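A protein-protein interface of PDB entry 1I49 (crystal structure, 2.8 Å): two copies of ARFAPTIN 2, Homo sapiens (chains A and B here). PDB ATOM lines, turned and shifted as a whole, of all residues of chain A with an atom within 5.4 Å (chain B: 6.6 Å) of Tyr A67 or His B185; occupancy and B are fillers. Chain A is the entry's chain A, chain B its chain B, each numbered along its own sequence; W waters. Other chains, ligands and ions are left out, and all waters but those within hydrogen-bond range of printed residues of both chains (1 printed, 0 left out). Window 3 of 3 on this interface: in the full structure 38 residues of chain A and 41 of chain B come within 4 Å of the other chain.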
ATOM      1  N   GLN A  62     -18.134  25.321 -18.039  1.00  0.00           N
ATOM      2  CA  GLN A  62     -18.367  25.569 -19.464  1.00  0.00           C
ATOM      3  C   GLN A  62     -17.265  25.111 -20.417  1.00  0.00           C
ATOM      4  O   GLN A  62     -17.539  24.712 -21.550  1.00  0.00           O
ATOM      5  CB  GLN A  62     -18.674  27.050 -19.707  1.00  0.00           C
ATOM      6  CG  GLN A  62     -17.516  28.004 -19.507  1.00  0.00           C
ATOM      7  CD  GLN A  62     -17.936  29.446 -19.716  1.00  0.00           C
ATOM      8  OE1 GLN A  62     -18.439  29.811 -20.784  1.00  0.00           O
ATOM      9  NE2 GLN A  62     -17.736  30.275 -18.694  1.00  0.00           N
ATOM     10  N   GLU A  63     -16.019  25.161 -19.968  1.00  0.00           N
ATOM     11  CA  GLU A  63     -14.929  24.726 -20.824  1.00  0.00           C
ATOM     12  C   GLU A  63     -15.073  23.223 -21.076  1.00  0.00           C
ATOM     13  O   GLU A  63     -15.400  22.793 -22.181  1.00  0.00           O
ATOM     14  CB  GLU A  63     -13.588  25.029 -20.157  1.00  0.00           C
ATOM     15  CG  GLU A  63     -12.492  25.416 -21.134  1.00  0.00           C
ATOM     16  CD  GLU A  63     -11.232  25.895 -20.439  1.00  0.00           C
ATOM     17  OE1 GLU A  63     -10.615  25.101 -19.691  1.00  0.00           O
ATOM     18  OE2 GLU A  63     -10.863  27.072 -20.644  1.00  0.00           O
ATOM     19  N   GLU A  64     -14.845  22.433 -20.034  1.00  0.00           N
ATOM     20  CA  GLU A  64     -14.944  20.984 -20.129  1.00  0.00           C
ATOM     21  C   GLU A  64     -16.153  20.499 -20.933  1.00  0.00           C
ATOM     22  O   GLU A  64     -16.019  19.647 -21.804  1.00  0.00           O
ATOM     23  CB  GLU A  64     -14.975  20.391 -18.738  1.00  0.00           C
ATOM     24  CG  GLU A  64     -13.757  20.753 -17.899  1.00  0.00           C
ATOM     25  CD  GLU A  64     -13.911  22.048 -17.083  1.00  0.00           C
ATOM     26  OE1 GLU A  64     -13.169  22.163 -16.078  1.00  0.00           O
ATOM     27  OE2 GLU A  64     -14.739  22.940 -17.430  1.00  0.00           O
ATOM     28  N   PHE A  65     -17.332  21.035 -20.649  1.00  0.00           N
ATOM     29  CA  PHE A  65     -18.518  20.631 -21.398  1.00  0.00           C
ATOM     30  C   PHE A  65     -18.441  21.014 -22.878  1.00  0.00           C
ATOM     31  O   PHE A  65     -18.757  20.195 -23.741  1.00  0.00           O
ATOM     32  CB  PHE A  65     -19.793  21.231 -20.784  1.00  0.00           C
ATOM     33  CG  PHE A  65     -20.354  20.423 -19.648  1.00  0.00           C
ATOM     34  CD1 PHE A  65     -20.140  20.803 -18.328  1.00  0.00           C
ATOM     35  CD2 PHE A  65     -21.068  19.257 -19.901  1.00  0.00           C
ATOM     36  CE1 PHE A  65     -20.630  20.030 -17.280  1.00  0.00           C
ATOM     37  CE2 PHE A  65     -21.560  18.480 -18.862  1.00  0.00           C
ATOM     38  CZ  PHE A  65     -21.341  18.864 -17.551  1.00  0.00           C
ATOM     39  N   GLY A  66     -18.028  22.250 -23.169  1.00  0.00           N
ATOM     40  CA  GLY A  66     -17.928  22.710 -24.553  1.00  0.00           C
ATOM     41  C   GLY A  66     -16.809  22.046 -25.341  1.00  0.00           C
ATOM     42  O   GLY A  66     -16.905  21.848 -26.549  1.00  0.00           O
ATOM     43  N   TYR A  67     -15.736  21.722 -24.632  1.00  0.00           N
ATOM     44  CA  TYR A  67     -14.560  21.049 -25.164  1.00  0.00           C
ATOM     45  C   TYR A  67     -15.056  19.708 -25.714  1.00  0.00           C
ATOM     46  O   TYR A  67     -14.904  19.406 -26.896  1.00  0.00           O
ATOM     47  CB  TYR A  67     -13.609  20.855 -23.985  1.00  0.00           C
ATOM     48  CG  TYR A  67     -12.259  20.258 -24.243  1.00  0.00           C
ATOM     49  CD1 TYR A  67     -11.477  20.669 -25.316  1.00  0.00           C
ATOM     50  CD2 TYR A  67     -11.705  19.365 -23.327  1.00  0.00           C
ATOM     51  CE1 TYR A  67     -10.159  20.210 -25.469  1.00  0.00           C
ATOM     52  CE2 TYR A  67     -10.395  18.904 -23.466  1.00  0.00           C
ATOM     53  CZ  TYR A  67      -9.626  19.330 -24.538  1.00  0.00           C
ATOM     54  OH  TYR A  67      -8.331  18.883 -24.669  1.00  0.00           O
ATOM     55  N   ASN A  68     -15.678  18.923 -24.837  1.00  0.00           N
ATOM     56  CA  ASN A  68     -16.220  17.618 -25.187  1.00  0.00           C
ATOM     57  C   ASN A  68     -17.345  17.738 -26.211  1.00  0.00           C
ATOM     58  O   ASN A  68     -17.523  16.850 -27.052  1.00  0.00           O
ATOM     59  CB  ASN A  68     -16.740  16.914 -23.931  1.00  0.00           C
ATOM     60  CG  ASN A  68     -15.624  16.353 -23.069  1.00  0.00           C
ATOM     61  OD1 ASN A  68     -15.050  15.311 -23.377  1.00  0.00           O
ATOM     62  ND2 ASN A  68     -15.300  17.052 -21.988  1.00  0.00           N
ATOM     63  N   ALA A  69     -18.104  18.828 -26.144  1.00  0.00           N
ATOM     64  CA  ALA A  69     -19.211  19.031 -27.080  1.00  0.00           C
ATOM     65  C   ALA A  69     -18.669  19.248 -28.489  1.00  0.00           C
ATOM     66  O   ALA A  69     -19.375  19.055 -29.484  1.00  0.00           O
ATOM     67  CB  ALA A  69     -20.074  20.238 -26.652  1.00  0.00           C
ATOM     68  N   GLU A  70     -17.404  19.651 -28.567  1.00  0.00           N
ATOM     69  CA  GLU A  70     -16.769  19.890 -29.851  1.00  0.00           C
ATOM     70  C   GLU A  70     -16.383  18.578 -30.520  1.00  0.00           C
ATOM     71  O   GLU A  70     -16.821  18.300 -31.645  1.00  0.00           O
ATOM     72  CB  GLU A  70     -15.545  20.795 -29.678  1.00  0.00           C
ATOM     73  CG  GLU A  70     -15.904  22.246 -29.428  1.00  0.00           C
ATOM     74  CD  GLU A  70     -16.895  22.786 -30.452  1.00  0.00           C
ATOM     75  OE1 GLU A  70     -17.987  22.195 -30.602  1.00  0.00           O
ATOM     76  OE2 GLU A  70     -16.585  23.805 -31.106  1.00  0.00           O
ATOM     77  N   THR A  71     -15.568  17.776 -29.837  1.00  0.00           N
ATOM     78  CA  THR A  71     -15.162  16.482 -30.372  1.00  0.00           C
ATOM     79  C   THR A  71     -16.405  15.717 -30.844  1.00  0.00           C
ATOM     80  O   THR A  71     -16.498  15.304 -31.997  1.00  0.00           O
ATOM     81  CB  THR A  71     -14.452  15.647 -29.300  1.00  0.00           C
ATOM     82  OG1 THR A  71     -13.259  16.324 -28.888  1.00  0.00           O
ATOM     83  CG2 THR A  71     -14.113  14.254 -29.836  1.00  0.00           C
ATOM     84  N   THR A 202      -7.615  21.472 -31.956  1.00  0.00           N
ATOM     85  CA  THR A 202      -8.404  21.930 -30.816  1.00  0.00           C
ATOM     86  C   THR A 202      -8.313  20.903 -29.690  1.00  0.00           C
ATOM     87  O   THR A 202      -7.671  21.210 -28.660  1.00  0.00           O
ATOM     88  CB  THR A 202      -9.889  22.116 -31.203  1.00  0.00           C
ATOM     89  OG1 THR A 202      -9.967  22.669 -32.518  1.00  0.00           O
ATOM     90  CG2 THR A 202     -10.586  23.085 -30.251  1.00  0.00           C
ATOM     91  N   GLN B 180     -13.349  13.639 -14.633  1.00  0.00           N
ATOM     92  CA  GLN B 180     -13.980  12.708 -15.560  1.00  0.00           C
ATOM     93  C   GLN B 180     -14.195  13.297 -16.949  1.00  0.00           C
ATOM     94  O   GLN B 180     -13.975  12.619 -17.954  1.00  0.00           O
ATOM     95  CB  GLN B 180     -15.337  12.245 -15.020  1.00  0.00           C
ATOM     96  CG  GLN B 180     -15.317  11.585 -13.655  1.00  0.00           C
ATOM     97  CD  GLN B 180     -14.577  10.270 -13.629  1.00  0.00           C
ATOM     98  OE1 GLN B 180     -14.835   9.383 -14.435  1.00  0.00           O
ATOM     99  NE2 GLN B 180     -13.659  10.128 -12.685  1.00  0.00           N
ATOM    100  N   LEU B 181     -14.637  14.547 -17.012  1.00  0.00           N
ATOM    101  CA  LEU B 181     -14.906  15.179 -18.302  1.00  0.00           C
ATOM    102  C   LEU B 181     -13.602  15.344 -19.068  1.00  0.00           C
ATOM    103  O   LEU B 181     -13.585  15.566 -20.286  1.00  0.00           O
ATOM    104  CB  LEU B 181     -15.598  16.530 -18.076  1.00  0.00           C
ATOM    105  CG  LEU B 181     -16.777  16.925 -18.984  1.00  0.00           C
ATOM    106  CD1 LEU B 181     -17.536  15.695 -19.452  1.00  0.00           C
ATOM    107  CD2 LEU B 181     -17.716  17.863 -18.227  1.00  0.00           C
ATOM    108  N   LEU B 182     -12.506  15.194 -18.330  1.00  0.00           N
ATOM    109  CA  LEU B 182     -11.152  15.319 -18.858  1.00  0.00           C
ATOM    110  C   LEU B 182     -10.681  13.964 -19.371  1.00  0.00           C
ATOM    111  O   LEU B 182     -10.395  13.811 -20.555  1.00  0.00           O
ATOM    112  CB  LEU B 182     -10.221  15.808 -17.747  1.00  0.00           C
ATOM    113  CG  LEU B 182      -8.824  16.328 -18.089  1.00  0.00           C
ATOM    114  CD1 LEU B 182      -8.927  17.704 -18.745  1.00  0.00           C
ATOM    115  CD2 LEU B 182      -7.995  16.401 -16.807  1.00  0.00           C
ATOM    116  N   LEU B 183     -10.603  12.983 -18.479  1.00  0.00           N
ATOM    117  CA  LEU B 183     -10.178  11.644 -18.869  1.00  0.00           C
ATOM    118  C   LEU B 183     -10.959  11.181 -20.091  1.00  0.00           C
ATOM    119  O   LEU B 183     -10.425  10.512 -20.970  1.00  0.00           O
ATOM    120  CB  LEU B 183     -10.420  10.653 -17.734  1.00  0.00           C
ATOM    121  CG  LEU B 183      -9.733  10.948 -16.413  1.00  0.00           C
ATOM    122  CD1 LEU B 183      -9.880   9.756 -15.492  1.00  0.00           C
ATOM    123  CD2 LEU B 183      -8.265  11.243 -16.665  1.00  0.00           C
ATOM    124  N   PHE B 184     -12.234  11.543 -20.138  1.00  0.00           N
ATOM    125  CA  PHE B 184     -13.074  11.152 -21.251  1.00  0.00           C
ATOM    126  C   PHE B 184     -12.621  11.760 -22.566  1.00  0.00           C
ATOM    127  O   PHE B 184     -12.469  11.054 -23.555  1.00  0.00           O
ATOM    128  CB  PHE B 184     -14.521  11.557 -21.014  1.00  0.00           C
ATOM    129  CG  PHE B 184     -15.443  11.128 -22.115  1.00  0.00           C
ATOM    130  CD1 PHE B 184     -15.814   9.791 -22.243  1.00  0.00           C
ATOM    131  CD2 PHE B 184     -15.931  12.054 -23.034  1.00  0.00           C
ATOM    132  CE1 PHE B 184     -16.659   9.390 -23.264  1.00  0.00           C
ATOM    133  CE2 PHE B 184     -16.782  11.663 -24.068  1.00  0.00           C
ATOM    134  CZ  PHE B 184     -17.149  10.336 -24.184  1.00  0.00           C
ATOM    135  N   HIS B 185     -12.438  13.074 -22.589  1.00  0.00           N
ATOM    136  CA  HIS B 185     -12.007  13.718 -23.818  1.00  0.00           C
ATOM    137  C   HIS B 185     -10.628  13.217 -24.215  1.00  0.00           C
ATOM    138  O   HIS B 185     -10.300  13.190 -25.400  1.00  0.00           O
ATOM    139  CB  HIS B 185     -11.969  15.230 -23.663  1.00  0.00           C
ATOM    140  CG  HIS B 185     -11.576  15.950 -24.914  1.00  0.00           C
ATOM    141  ND1 HIS B 185     -12.474  16.673 -25.672  1.00  0.00           N
ATOM    142  CD2 HIS B 185     -10.378  16.076 -25.532  1.00  0.00           C
ATOM    143  CE1 HIS B 185     -11.848  17.214 -26.700  1.00  0.00           C
ATOM    144  NE2 HIS B 185     -10.575  16.867 -26.639  1.00  0.00           N
ATOM    145  N   ASN B 186      -9.814  12.827 -23.236  1.00  0.00           N
ATOM    146  CA  ASN B 186      -8.488  12.314 -23.559  1.00  0.00           C
ATOM    147  C   ASN B 186      -8.630  10.946 -24.186  1.00  0.00           C
ATOM    148  O   ASN B 186      -8.145  10.706 -25.283  1.00  0.00           O
ATOM    149  CB  ASN B 186      -7.609  12.211 -22.320  1.00  0.00           C
ATOM    150  CG  ASN B 186      -7.147  13.562 -21.830  1.00  0.00           C
ATOM    151  OD1 ASN B 186      -7.155  14.544 -22.579  1.00  0.00           O
ATOM    152  ND2 ASN B 186      -6.730  13.622 -20.570  1.00  0.00           N
ATOM    153  N   ALA B 187      -9.305  10.048 -23.481  1.00  0.00           N
ATOM    154  CA  ALA B 187      -9.526   8.699 -23.979  1.00  0.00           C
ATOM    155  C   ALA B 187      -9.982   8.748 -25.443  1.00  0.00           C
ATOM    156  O   ALA B 187      -9.429   8.072 -26.303  1.00  0.00           O
ATOM    157  CB  ALA B 187     -10.574   7.998 -23.109  1.00  0.00           C
ATOM    158  N   VAL B 188     -10.992   9.563 -25.712  1.00  0.00           N
ATOM    159  CA  VAL B 188     -11.526   9.715 -27.052  1.00  0.00           C
ATOM    160  C   VAL B 188     -10.442  10.114 -28.025  1.00  0.00           C
ATOM    161  O   VAL B 188     -10.317   9.509 -29.086  1.00  0.00           O
ATOM    162  CB  VAL B 188     -12.616  10.803 -27.111  1.00  0.00           C
ATOM    163  CG1 VAL B 188     -12.917  11.161 -28.573  1.00  0.00           C
ATOM    164  CG2 VAL B 188     -13.874  10.323 -26.399  1.00  0.00           C
ATOM    165  N   SER B 189      -9.664  11.137 -27.679  1.00  0.00           N
ATOM    166  CA  SER B 189      -8.598  11.591 -28.573  1.00  0.00           C
ATOM    167  C   SER B 189      -7.440  10.587 -28.623  1.00  0.00           C
ATOM    168  O   SER B 189      -6.805  10.425 -29.662  1.00  0.00           O
ATOM    169  CB  SER B 189      -8.073  12.969 -28.148  1.00  0.00           C
ATOM    170  OG  SER B 189      -6.953  12.849 -27.291  1.00  0.00           O
ATOM    171  N   ALA B 190      -7.176   9.916 -27.505  1.00  0.00           N
ATOM    172  CA  ALA B 190      -6.106   8.927 -27.436  1.00  0.00           C
ATOM    173  C   ALA B 190      -6.395   7.770 -28.392  1.00  0.00           C
ATOM    174  O   ALA B 190      -5.481   7.162 -28.951  1.00  0.00           O
ATOM    175  CB  ALA B 190      -5.970   8.407 -26.019  1.00  0.00           C
HETATM  176  O   HOH W   1      -7.565  16.429 -24.276  1.00  0.00           O
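Glu A64 touches Leu B181 (CB to CD2, 3.8 Å). Phe A65 touches Leu B181. His B185 touches Tyr A67 (NE2 to CZ, 3.4 Å). Phe B184 touches Asn A68 (CD2 to OD1, 3.4 Å). Asn A68 touches His B185. CG1 of Val B188 touches CG2 of Thr A71 (3.5 Å).
Water W1 lies within hydrogen-bond range of the side-chain amide oxygen of Asn B186 and the side-chain hydroxyl of Tyr A67.
Of the 11 printed residues of chain A, 5 touch a printed residue of chain B. Printed residues of chain A that touch a printed residue of chain B: Glu A64, Phe A65, Tyr A67, Asn A68 and Thr A71. Printed residues of chain B that touch a printed residue of chain A: Leu B181, Phe B184, His B185 and Val B188. Among the printed residues, no Asp or Glu carboxylate lies within 4 Å of a Lys or Arg side-chain nitrogen of the other chain.
ND2 of Asn A68 is in hydrogen-bond range of O of Leu B181 (2.8 Å). OG1 of Thr A71 sits close to ND1 of His B185 (3.3 Å).
No position is printed for both chains.
Tyr A67 touches just one residue of chain B: His B185. Printed residues of chain A within 4 Å of His B185: Tyr A67 (3.4 Å), Asn A68 (3.1 Å) and Thr A71 (2.8 Å). Of the printed residues of chain A, Val B188 touches Thr A71. Of the printed residues of chain B, Asn A68 touches Leu B181, Phe B184 and His B185. Printed residues of chain B within 4 Å of Thr A71: His B185 (2.8 Å) and Val B188 (3.5 Å). Printed residues of chain B within 4 Å of Glu A64: Leu B181 (3.8 Å). Of the printed residues of chain A, Leu B181 touches Glu A64 (3.8 Å), Phe A65 (3.8 Å) and Asn A68 (2.8 Å). Gln A62 touches none of the printed residues of chain B. Asn B186 touches none of the printed residues of chain A.
The side-chain amide nitrogen (ND2) of Asn A68 sits at hydrogen-bond distance from the backbone carbonyl oxygen (O) of Glu A64.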
